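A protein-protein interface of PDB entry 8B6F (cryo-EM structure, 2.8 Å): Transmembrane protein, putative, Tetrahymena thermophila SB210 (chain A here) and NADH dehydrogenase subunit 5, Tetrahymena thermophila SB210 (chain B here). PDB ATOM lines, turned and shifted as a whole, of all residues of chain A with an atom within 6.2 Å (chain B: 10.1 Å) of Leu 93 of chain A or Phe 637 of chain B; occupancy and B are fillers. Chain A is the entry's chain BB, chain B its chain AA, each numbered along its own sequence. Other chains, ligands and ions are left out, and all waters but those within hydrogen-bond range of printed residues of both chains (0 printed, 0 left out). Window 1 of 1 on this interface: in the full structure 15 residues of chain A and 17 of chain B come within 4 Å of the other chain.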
ATOM      1  N   PRO A  89      14.270  11.415  21.157  1.00  0.00           N
ATOM      2  CA  PRO A  89      13.280  10.802  22.043  1.00  0.00           C
ATOM      3  C   PRO A  89      12.334   9.919  21.249  1.00  0.00           C
ATOM      4  O   PRO A  89      12.128  10.110  20.048  1.00  0.00           O
ATOM      5  CB  PRO A  89      12.550  12.002  22.654  1.00  0.00           C
ATOM      6  CG  PRO A  89      12.735  13.093  21.671  1.00  0.00           C
ATOM      7  CD  PRO A  89      14.081  12.873  21.052  1.00  0.00           C
ATOM      8  N   TYR A  90      11.760   8.936  21.934  1.00  0.00           N
ATOM      9  CA  TYR A  90      10.882   7.938  21.336  1.00  0.00           C
ATOM     10  C   TYR A  90      11.634   6.983  20.424  1.00  0.00           C
ATOM     11  O   TYR A  90      11.005   6.261  19.643  1.00  0.00           O
ATOM     12  CB  TYR A  90       9.738   8.592  20.553  1.00  0.00           C
ATOM     13  CG  TYR A  90       9.117   9.770  21.268  1.00  0.00           C
ATOM     14  CD1 TYR A  90       8.358   9.589  22.414  1.00  0.00           C
ATOM     15  CD2 TYR A  90       9.285  11.061  20.788  1.00  0.00           C
ATOM     16  CE1 TYR A  90       7.790  10.660  23.069  1.00  0.00           C
ATOM     17  CE2 TYR A  90       8.720  12.140  21.436  1.00  0.00           C
ATOM     18  CZ  TYR A  90       7.971  11.933  22.574  1.00  0.00           C
ATOM     19  OH  TYR A  90       7.405  13.003  23.224  1.00  0.00           O
ATOM     20  N   HIS A  91      12.966   6.956  20.499  1.00  0.00           N
ATOM     21  CA  HIS A  91      13.734   5.979  19.736  1.00  0.00           C
ATOM     22  C   HIS A  91      13.292   4.563  20.070  1.00  0.00           C
ATOM     23  O   HIS A  91      13.182   3.708  19.184  1.00  0.00           O
ATOM     24  CB  HIS A  91      15.226   6.154  20.011  1.00  0.00           C
ATOM     25  CG  HIS A  91      16.082   5.107  19.370  1.00  0.00           C
ATOM     26  ND1 HIS A  91      16.681   4.094  20.087  1.00  0.00           N
ATOM     27  CD2 HIS A  91      16.436   4.913  18.078  1.00  0.00           C
ATOM     28  CE1 HIS A  91      17.369   3.323  19.265  1.00  0.00           C
ATOM     29  NE2 HIS A  91      17.236   3.798  18.040  1.00  0.00           N
ATOM     30  N   HIS A  92      13.032   4.297  21.351  1.00  0.00           N
ATOM     31  CA  HIS A  92      12.494   3.001  21.745  1.00  0.00           C
ATOM     32  C   HIS A  92      11.144   2.735  21.095  1.00  0.00           C
ATOM     33  O   HIS A  92      10.817   1.581  20.802  1.00  0.00           O
ATOM     34  CB  HIS A  92      12.379   2.929  23.268  1.00  0.00           C
ATOM     35  CG  HIS A  92      11.551   4.024  23.866  1.00  0.00           C
ATOM     36  ND1 HIS A  92      10.273   3.816  24.340  1.00  0.00           N
ATOM     37  CD2 HIS A  92      11.817   5.335  24.067  1.00  0.00           C
ATOM     38  CE1 HIS A  92       9.789   4.953  24.806  1.00  0.00           C
ATOM     39  NE2 HIS A  92      10.706   5.890  24.654  1.00  0.00           N
ATOM     40  N   LEU A  93      10.344   3.779  20.868  1.00  0.00           N
ATOM     41  CA  LEU A  93       9.037   3.599  20.245  1.00  0.00           C
ATOM     42  C   LEU A  93       9.132   3.362  18.745  1.00  0.00           C
ATOM     43  O   LEU A  93       8.240   2.729  18.171  1.00  0.00           O
ATOM     44  CB  LEU A  93       8.155   4.817  20.513  1.00  0.00           C
ATOM     45  CG  LEU A  93       7.782   5.069  21.974  1.00  0.00           C
ATOM     46  CD1 LEU A  93       6.907   6.296  22.096  1.00  0.00           C
ATOM     47  CD2 LEU A  93       7.083   3.860  22.577  1.00  0.00           C
ATOM     48  N   ARG A  94      10.179   3.861  18.092  1.00  0.00           N
ATOM     49  CA  ARG A  94      10.307   3.699  16.649  1.00  0.00           C
ATOM     50  C   ARG A  94      10.214   2.229  16.266  1.00  0.00           C
ATOM     51  O   ARG A  94      10.968   1.394  16.769  1.00  0.00           O
ATOM     52  CB  ARG A  94      11.638   4.279  16.163  1.00  0.00           C
ATOM     53  CG  ARG A  94      11.877   5.734  16.538  1.00  0.00           C
ATOM     54  CD  ARG A  94      10.843   6.667  15.940  1.00  0.00           C
ATOM     55  NE  ARG A  94      11.048   8.038  16.388  1.00  0.00           N
ATOM     56  CZ  ARG A  94      10.254   9.055  16.083  1.00  0.00           C
ATOM     57  NH1 ARG A  94       9.188   8.892  15.318  1.00  0.00           N
ATOM     58  NH2 ARG A  94      10.538  10.265  16.553  1.00  0.00           N
ATOM     59  N   GLY A  95       9.286   1.920  15.362  1.00  0.00           N
ATOM     60  CA  GLY A  95       9.120   0.564  14.876  1.00  0.00           C
ATOM     61  C   GLY A  95       8.690  -0.428  15.939  1.00  0.00           C
ATOM     62  O   GLY A  95       9.257  -1.519  16.040  1.00  0.00           O
ATOM     63  N   VAL A  96       7.692  -0.062  16.737  1.00  0.00           N
ATOM     64  CA  VAL A  96       7.178  -0.932  17.792  1.00  0.00           C
ATOM     65  C   VAL A  96       5.673  -1.095  17.604  1.00  0.00           C
ATOM     66  O   VAL A  96       4.993  -0.123  17.248  1.00  0.00           O
ATOM     67  CB  VAL A  96       7.510  -0.362  19.181  1.00  0.00           C
ATOM     68  CG1 VAL A  96       6.960  -1.242  20.274  1.00  0.00           C
ATOM     69  CG2 VAL A  96       9.006  -0.217  19.345  1.00  0.00           C
ATOM     70  N   PRO A  97       5.108  -2.283  17.824  1.00  0.00           N
ATOM     71  CA  PRO A  97       3.654  -2.436  17.690  1.00  0.00           C
ATOM     72  C   PRO A  97       2.897  -1.632  18.734  1.00  0.00           C
ATOM     73  O   PRO A  97       3.396  -1.357  19.827  1.00  0.00           O
ATOM     74  CB  PRO A  97       3.434  -3.942  17.883  1.00  0.00           C
ATOM     75  CG  PRO A  97       4.625  -4.410  18.628  1.00  0.00           C
ATOM     76  CD  PRO A  97       5.759  -3.565  18.144  1.00  0.00           C
ATOM     77  N   GLU A 102       6.102  -0.972  25.715  1.00  0.00           N
ATOM     78  CA  GLU A 102       6.776   0.285  25.406  1.00  0.00           C
ATOM     79  C   GLU A 102       5.778   1.357  24.986  1.00  0.00           C
ATOM     80  O   GLU A 102       5.813   2.486  25.486  1.00  0.00           O
ATOM     81  CB  GLU A 102       7.819   0.072  24.308  1.00  0.00           C
ATOM     82  CG  GLU A 102       9.055  -0.700  24.747  1.00  0.00           C
ATOM     83  CD  GLU A 102       8.797  -2.184  24.920  1.00  0.00           C
ATOM     84  OE1 GLU A 102       7.735  -2.663  24.471  1.00  0.00           O
ATOM     85  OE2 GLU A 102       9.658  -2.873  25.505  1.00  0.00           O
ATOM     86  N   ARG A 103       4.875   1.019  24.064  1.00  0.00           N
ATOM     87  CA  ARG A 103       3.915   2.007  23.582  1.00  0.00           C
ATOM     88  C   ARG A 103       2.847   2.304  24.627  1.00  0.00           C
ATOM     89  O   ARG A 103       2.498   3.468  24.853  1.00  0.00           O
ATOM     90  CB  ARG A 103       3.269   1.520  22.285  1.00  0.00           C
ATOM     91  CG  ARG A 103       2.302   2.517  21.659  1.00  0.00           C
ATOM     92  CD  ARG A 103       3.017   3.775  21.198  1.00  0.00           C
ATOM     93  NE  ARG A 103       2.097   4.742  20.611  1.00  0.00           N
ATOM     94  CZ  ARG A 103       1.449   5.679  21.292  1.00  0.00           C
ATOM     95  NH1 ARG A 103       1.579   5.798  22.603  1.00  0.00           N
ATOM     96  NH2 ARG A 103       0.652   6.520  20.639  1.00  0.00           N
ATOM     97  N   MET A 104       2.314   1.266  25.269  1.00  0.00           N
ATOM     98  CA  MET A 104       1.172   1.453  26.156  1.00  0.00           C
ATOM     99  C   MET A 104       1.567   2.192  27.429  1.00  0.00           C
ATOM    100  O   MET A 104       0.898   3.150  27.831  1.00  0.00           O
ATOM    101  CB  MET A 104       0.552   0.098  26.493  1.00  0.00           C
ATOM    102  CG  MET A 104      -0.209  -0.536  25.341  1.00  0.00           C
ATOM    103  SD  MET A 104      -1.664   0.418  24.870  1.00  0.00           S
ATOM    104  CE  MET A 104      -2.304  -0.571  23.523  1.00  0.00           C
ATOM    105  N   PHE A 106       5.330   2.664  28.696  1.00  0.00           N
ATOM    106  CA  PHE A 106       6.647   3.285  28.767  1.00  0.00           C
ATOM    107  C   PHE A 106       6.939   4.166  27.559  1.00  0.00           C
ATOM    108  O   PHE A 106       8.097   4.291  27.150  1.00  0.00           O
ATOM    109  CB  PHE A 106       7.723   2.209  28.911  1.00  0.00           C
ATOM    110  CG  PHE A 106       7.443   1.211  29.998  1.00  0.00           C
ATOM    111  CD1 PHE A 106       6.797   1.594  31.164  1.00  0.00           C
ATOM    112  CD2 PHE A 106       7.816  -0.113  29.850  1.00  0.00           C
ATOM    113  CE1 PHE A 106       6.536   0.675  32.161  1.00  0.00           C
ATOM    114  CE2 PHE A 106       7.556  -1.037  30.842  1.00  0.00           C
ATOM    115  CZ  PHE A 106       6.915  -0.642  32.000  1.00  0.00           C
ATOM    116  N   ALA A 107       5.913   4.780  26.980  1.00  0.00           N
ATOM    117  CA  ALA A 107       6.082   5.640  25.810  1.00  0.00           C
ATOM    118  C   ALA A 107       6.455   7.063  26.208  1.00  0.00           C
ATOM    119  O   ALA A 107       5.809   8.032  25.815  1.00  0.00           O
ATOM    120  CB  ALA A 107       4.808   5.623  24.975  1.00  0.00           C
ATOM    121  N   ASP A 108       7.520   7.196  26.992  1.00  0.00           N
ATOM    122  CA  ASP A 108       7.983   8.486  27.472  1.00  0.00           C
ATOM    123  C   ASP A 108       9.083   9.022  26.562  1.00  0.00           C
ATOM    124  O   ASP A 108       9.514   8.373  25.607  1.00  0.00           O
ATOM    125  CB  ASP A 108       8.462   8.370  28.919  1.00  0.00           C
ATOM    126  CG  ASP A 108       7.318   8.203  29.893  1.00  0.00           C
ATOM    127  OD1 ASP A 108       6.399   9.047  29.881  1.00  0.00           O
ATOM    128  OD2 ASP A 108       7.324   7.220  30.659  1.00  0.00           O
ATOM    129  N   ARG B 277       4.682   3.878  37.120  1.00  0.00           N
ATOM    130  CA  ARG B 277       5.678   3.660  36.086  1.00  0.00           C
ATOM    131  C   ARG B 277       7.053   4.118  36.557  1.00  0.00           C
ATOM    132  O   ARG B 277       7.202   5.213  37.107  1.00  0.00           O
ATOM    133  CB  ARG B 277       5.247   4.428  34.838  1.00  0.00           C
ATOM    134  CG  ARG B 277       6.116   4.267  33.618  1.00  0.00           C
ATOM    135  CD  ARG B 277       5.927   5.466  32.702  1.00  0.00           C
ATOM    136  NE  ARG B 277       4.530   5.882  32.647  1.00  0.00           N
ATOM    137  CZ  ARG B 277       4.117   7.087  32.282  1.00  0.00           C
ATOM    138  NH1 ARG B 277       4.969   8.033  31.926  1.00  0.00           N
ATOM    139  NH2 ARG B 277       2.815   7.355  32.281  1.00  0.00           N
ATOM    140  N   TYR B 278       8.062   3.272  36.338  1.00  0.00           N
ATOM    141  CA  TYR B 278       9.452   3.570  36.686  1.00  0.00           C
ATOM    142  C   TYR B 278       9.665   3.664  38.192  1.00  0.00           C
ATOM    143  O   TYR B 278      10.581   4.348  38.650  1.00  0.00           O
ATOM    144  CB  TYR B 278       9.928   4.864  36.021  1.00  0.00           C
ATOM    145  CG  TYR B 278       9.666   4.925  34.540  1.00  0.00           C
ATOM    146  CD1 TYR B 278       9.655   3.772  33.766  1.00  0.00           C
ATOM    147  CD2 TYR B 278       9.427   6.139  33.913  1.00  0.00           C
ATOM    148  CE1 TYR B 278       9.411   3.827  32.411  1.00  0.00           C
ATOM    149  CE2 TYR B 278       9.183   6.205  32.561  1.00  0.00           C
ATOM    150  CZ  TYR B 278       9.175   5.045  31.813  1.00  0.00           C
ATOM    151  OH  TYR B 278       8.935   5.108  30.462  1.00  0.00           O
ATOM    152  N   ILE B 632      11.685  19.509  20.607  1.00  0.00           N
ATOM    153  CA  ILE B 632      12.203  18.184  20.279  1.00  0.00           C
ATOM    154  C   ILE B 632      11.179  17.108  20.612  1.00  0.00           C
ATOM    155  O   ILE B 632      11.142  16.053  19.969  1.00  0.00           O
ATOM    156  CB  ILE B 632      13.536  17.940  21.014  1.00  0.00           C
ATOM    157  CG1 ILE B 632      14.153  16.599  20.606  1.00  0.00           C
ATOM    158  CG2 ILE B 632      13.335  17.981  22.524  1.00  0.00           C
ATOM    159  CD1 ILE B 632      14.612  16.542  19.169  1.00  0.00           C
ATOM    160  N   LEU B 633      10.334  17.352  21.614  1.00  0.00           N
ATOM    161  CA  LEU B 633       9.348  16.367  22.034  1.00  0.00           C
ATOM    162  C   LEU B 633       8.171  16.256  21.075  1.00  0.00           C
ATOM    163  O   LEU B 633       7.421  15.278  21.155  1.00  0.00           O
ATOM    164  CB  LEU B 633       8.834  16.713  23.432  1.00  0.00           C
ATOM    165  CG  LEU B 633       9.898  16.773  24.528  1.00  0.00           C
ATOM    166  CD1 LEU B 633       9.294  17.265  25.831  1.00  0.00           C
ATOM    167  CD2 LEU B 633      10.551  15.417  24.722  1.00  0.00           C
ATOM    168  N   ASN B 634       7.990  17.223  20.178  1.00  0.00           N
ATOM    169  CA  ASN B 634       6.867  17.189  19.250  1.00  0.00           C
ATOM    170  C   ASN B 634       6.923  15.922  18.411  1.00  0.00           C
ATOM    171  O   ASN B 634       7.827  15.756  17.587  1.00  0.00           O
ATOM    172  CB  ASN B 634       6.875  18.426  18.349  1.00  0.00           C
ATOM    173  CG  ASN B 634       5.599  18.567  17.545  1.00  0.00           C
ATOM    174  OD1 ASN B 634       4.924  17.581  17.251  1.00  0.00           O
ATOM    175  ND2 ASN B 634       5.259  19.799  17.186  1.00  0.00           N
ATOM    176  N   SER B 635       5.961  15.027  18.606  1.00  0.00           N
ATOM    177  CA  SER B 635       5.966  13.751  17.908  1.00  0.00           C
ATOM    178  C   SER B 635       4.569  13.156  17.952  1.00  0.00           C
ATOM    179  O   SER B 635       3.720  13.576  18.741  1.00  0.00           O
ATOM    180  CB  SER B 635       6.979  12.784  18.529  1.00  0.00           C
ATOM    181  OG  SER B 635       6.976  11.540  17.855  1.00  0.00           O
ATOM    182  N   LYS B 636       4.342  12.165  17.088  1.00  0.00           N
ATOM    183  CA  LYS B 636       3.084  11.430  17.126  1.00  0.00           C
ATOM    184  C   LYS B 636       2.904  10.692  18.442  1.00  0.00           C
ATOM    185  O   LYS B 636       1.767  10.403  18.828  1.00  0.00           O
ATOM    186  CB  LYS B 636       3.010  10.439  15.962  1.00  0.00           C
ATOM    187  CG  LYS B 636       4.049   9.331  16.024  1.00  0.00           C
ATOM    188  CD  LYS B 636       4.061   8.494  14.752  1.00  0.00           C
ATOM    189  CE  LYS B 636       2.797   7.663  14.595  1.00  0.00           C
ATOM    190  NZ  LYS B 636       2.634   6.661  15.684  1.00  0.00           N
ATOM    191  N   PHE B 637       3.996  10.376  19.134  1.00  0.00           N
ATOM    192  CA  PHE B 637       3.941   9.690  20.416  1.00  0.00           C
ATOM    193  C   PHE B 637       3.840  10.644  21.598  1.00  0.00           C
ATOM    194  O   PHE B 637       3.707  10.179  22.735  1.00  0.00           O
ATOM    195  CB  PHE B 637       5.182   8.810  20.596  1.00  0.00           C
ATOM    196  CG  PHE B 637       5.431   7.869  19.458  1.00  0.00           C
ATOM    197  CD1 PHE B 637       4.632   6.753  19.277  1.00  0.00           C
ATOM    198  CD2 PHE B 637       6.481   8.087  18.582  1.00  0.00           C
ATOM    199  CE1 PHE B 637       4.867   5.879  18.236  1.00  0.00           C
ATOM    200  CE2 PHE B 637       6.722   7.218  17.541  1.00  0.00           C
ATOM    201  CZ  PHE B 637       5.914   6.112  17.366  1.00  0.00           C
ATOM    202  N   TYR B 638       3.904  11.952  21.368  1.00  0.00           N
ATOM    203  CA  TYR B 638       3.946  12.897  22.474  1.00  0.00           C
ATOM    204  C   TYR B 638       2.714  12.757  23.357  1.00  0.00           C
ATOM    205  O   TYR B 638       1.584  12.691  22.866  1.00  0.00           O
ATOM    206  CB  TYR B 638       4.046  14.329  21.952  1.00  0.00           C
ATOM    207  CG  TYR B 638       3.986  15.362  23.052  1.00  0.00           C
ATOM    208  CD1 TYR B 638       5.139  15.782  23.698  1.00  0.00           C
ATOM    209  CD2 TYR B 638       2.774  15.906  23.455  1.00  0.00           C
ATOM    210  CE1 TYR B 638       5.088  16.720  24.709  1.00  0.00           C
ATOM    211  CE2 TYR B 638       2.712  16.843  24.465  1.00  0.00           C
ATOM    212  CZ  TYR B 638       3.873  17.246  25.087  1.00  0.00           C
ATOM    213  OH  TYR B 638       3.817  18.179  26.094  1.00  0.00           O
ATOM    214  N   SER B 639       2.942  12.711  24.665  1.00  0.00           N
ATOM    215  CA  SER B 639       1.873  12.726  25.652  1.00  0.00           C
ATOM    216  C   SER B 639       2.506  12.830  27.029  1.00  0.00           C
ATOM    217  O   SER B 639       3.602  12.315  27.260  1.00  0.00           O
ATOM    218  CB  SER B 639       0.992  11.475  25.559  1.00  0.00           C
ATOM    219  OG  SER B 639       1.756  10.296  25.742  1.00  0.00           O
ATOM    220  N   ASN B 640       1.808  13.506  27.935  1.00  0.00           N
ATOM    221  CA  ASN B 640       2.223  13.601  29.327  1.00  0.00           C
ATOM    222  C   ASN B 640       1.564  12.548  30.205  1.00  0.00           C
ATOM    223  O   ASN B 640       1.818  12.519  31.413  1.00  0.00           O
ATOM    224  CB  ASN B 640       1.918  14.995  29.874  1.00  0.00           C
ATOM    225  CG  ASN B 640       2.703  16.077  29.169  1.00  0.00           C
ATOM    226  OD1 ASN B 640       3.854  16.344  29.510  1.00  0.00           O
ATOM    227  ND2 ASN B 640       2.082  16.715  28.186  1.00  0.00           N
ATOM    228  N   THR B 641       0.727  11.690  29.628  1.00  0.00           N
ATOM    229  CA  THR B 641       0.126  10.580  30.351  1.00  0.00           C
ATOM    230  C   THR B 641       0.381   9.286  29.590  1.00  0.00           C
ATOM    231  O   THR B 641       1.163   9.268  28.634  1.00  0.00           O
ATOM    232  CB  THR B 641      -1.375  10.802  30.549  1.00  0.00           C
ATOM    233  OG1 THR B 641      -1.952   9.658  31.190  1.00  0.00           O
ATOM    234  CG2 THR B 641      -2.070  11.044  29.217  1.00  0.00           C
ATOM    235  N   SER B 642      -0.266   8.206  30.003  1.00  0.00           N
ATOM    236  CA  SER B 642      -0.087   6.899  29.389  1.00  0.00           C
ATOM    237  C   SER B 642      -1.286   6.558  28.517  1.00  0.00           C
ATOM    238  O   SER B 642      -2.433   6.815  28.891  1.00  0.00           O
ATOM    239  CB  SER B 642       0.105   5.824  30.461  1.00  0.00           C
ATOM    240  OG  SER B 642       0.307   4.550  29.878  1.00  0.00           O
ATOM    241  N   LEU B 643      -1.012   5.977  27.347  1.00  0.00           N
ATOM    242  CA  LEU B 643      -2.093   5.528  26.475  1.00  0.00           C
ATOM    243  C   LEU B 643      -2.939   4.469  27.164  1.00  0.00           C
ATOM    244  O   LEU B 643      -4.171   4.476  27.052  1.00  0.00           O
ATOM    245  CB  LEU B 643      -1.520   4.989  25.165  1.00  0.00           C
ATOM    246  CG  LEU B 643      -2.534   4.420  24.171  1.00  0.00           C
ATOM    247  CD1 LEU B 643      -3.555   5.471  23.789  1.00  0.00           C
ATOM    248  CD2 LEU B 643      -1.822   3.891  22.938  1.00  0.00           C
ATOM    249  N   ASN B 646      -5.204   6.273  29.560  1.00  0.00           N
ATOM    250  CA  ASN B 646      -6.335   6.907  28.893  1.00  0.00           C
ATOM    251  C   ASN B 646      -7.391   5.879  28.513  1.00  0.00           C
ATOM    252  O   ASN B 646      -8.588   6.096  28.726  1.00  0.00           O
ATOM    253  CB  ASN B 646      -5.855   7.663  27.656  1.00  0.00           C
ATOM    254  CG  ASN B 646      -4.841   8.735  27.989  1.00  0.00           C
ATOM    255  OD1 ASN B 646      -4.762   9.199  29.126  1.00  0.00           O
ATOM    256  ND2 ASN B 646      -4.057   9.137  26.997  1.00  0.00           N
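Pro 89 of chain A touches Ile 632 of chain B.
CE2 of Tyr 90 of chain A touches CB of Ser 635 of chain B, 3.4 Å away.
CB of Phe 637 of chain B touches CD1 of Tyr 90 of chain A (3.7 Å).
OH of Tyr 90 of chain A touches CA of Tyr 638 of chain B, at 3.5 Å.
CD1 of Leu 93 of chain A touches CB of Phe 637 of chain B (3.4 Å).
NH1 of Arg 94 of chain A touches CE2 of Phe 637 of chain B (3.7 Å).
Arg 103 of chain A touches Phe 637 of chain B (NE to CD1, 3.5 Å).
CD2 of Leu 643 of chain B touches NH1 of Arg 103 of chain A (3.9 Å).
CD1 of Phe 106 of chain A touches CG of Arg 277 of chain B, 3.7 Å away.
OH of Tyr 278 of chain B touches CA of Phe 106 of chain A (3.4 Å).
Of the 15 printed residues of chain A, 8 touch a printed residue of chain B.
Of chain B, only Phe 637 comes within 4 Å of Leu 93 of chain A.
No residue of chain B comes within 4 Å of His 92 of chain A.
No residue of chain B comes within 4 Å of Gly 95 of chain A.
Of chain B, only Phe 637 (3.5 Å) and Leu 643 (3.9 Å) come within 4 Å of Arg 103 of chain A.
Of the printed residues of chain A, Ile 632 of chain B touches Pro 89 (3.8 Å).
Of the printed residues of chain B, Pro 89 of chain A touches Ile 632 (3.8 Å).
Printed residues of chain A within 4 Å of Arg 277 of chain B: Phe 106 (3.7 Å) and Asp 108 (2.7 Å).
Of the printed residues of chain A, Ser 635 of chain B touches Tyr 90 (3.4 Å).
Of the printed residues of chain B, Asp 108 of chain A touches Arg 277 (2.7 Å) and Tyr 278 (2.7 Å).
His 91 of chain A touches none of the printed residues of chain B.
Thr 641 of chain B touches none of the printed residues of chain A.
The nearest residue of chain B that does not touch Leu 93 of chain A is Tyr 638 of chain B (6.4 Å).
NE2 of His 92 of chain A sits at hydrogen-bond distance from O of Asp 108 of chain A (2.9 Å).
The backbone NH (N) of Phe 637 of chain B lies close to the side-chain hydroxyl (OG) of Ser 635 of chain B (3.4 Å).
The side-chain amide oxygen of Asn 646 of chain B sits close to the backbone carbonyl oxygen of Ser 642 of chain B.
The side-chain hydroxyl (OH) of Tyr 638 of chain B lies within hydrogen-bond range of the side-chain amide nitrogen (ND2) of Asn 640 of chain B.
The side-chain hydroxyl (OH) of Tyr 278 of chain B is in hydrogen-bond range of the side-chain carboxylate (OD2) of Asp 108 of chain A, at 2.7 Å.
The guanidinium group (NH1) of Arg 277 of chain B is in salt-bridge range of the side-chain carboxylate (OD1) of Asp 108 of chain A (2.7 Å).
The backbone NH (N) of Leu 643 of chain B lies within hydrogen-bond range of the backbone carbonyl oxygen (O) of Met 104 of chain A, at 3.4 Å.
OG of Ser 642 of chain B lies within hydrogen-bond range of O of Met 104 of chain A (2.5 Å).
The side-chain hydroxyl of Tyr 90 of chain A sits at hydrogen-bond distance from the backbone carbonyl oxygen of Leu 633 of chain B, 3.1 Å away.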
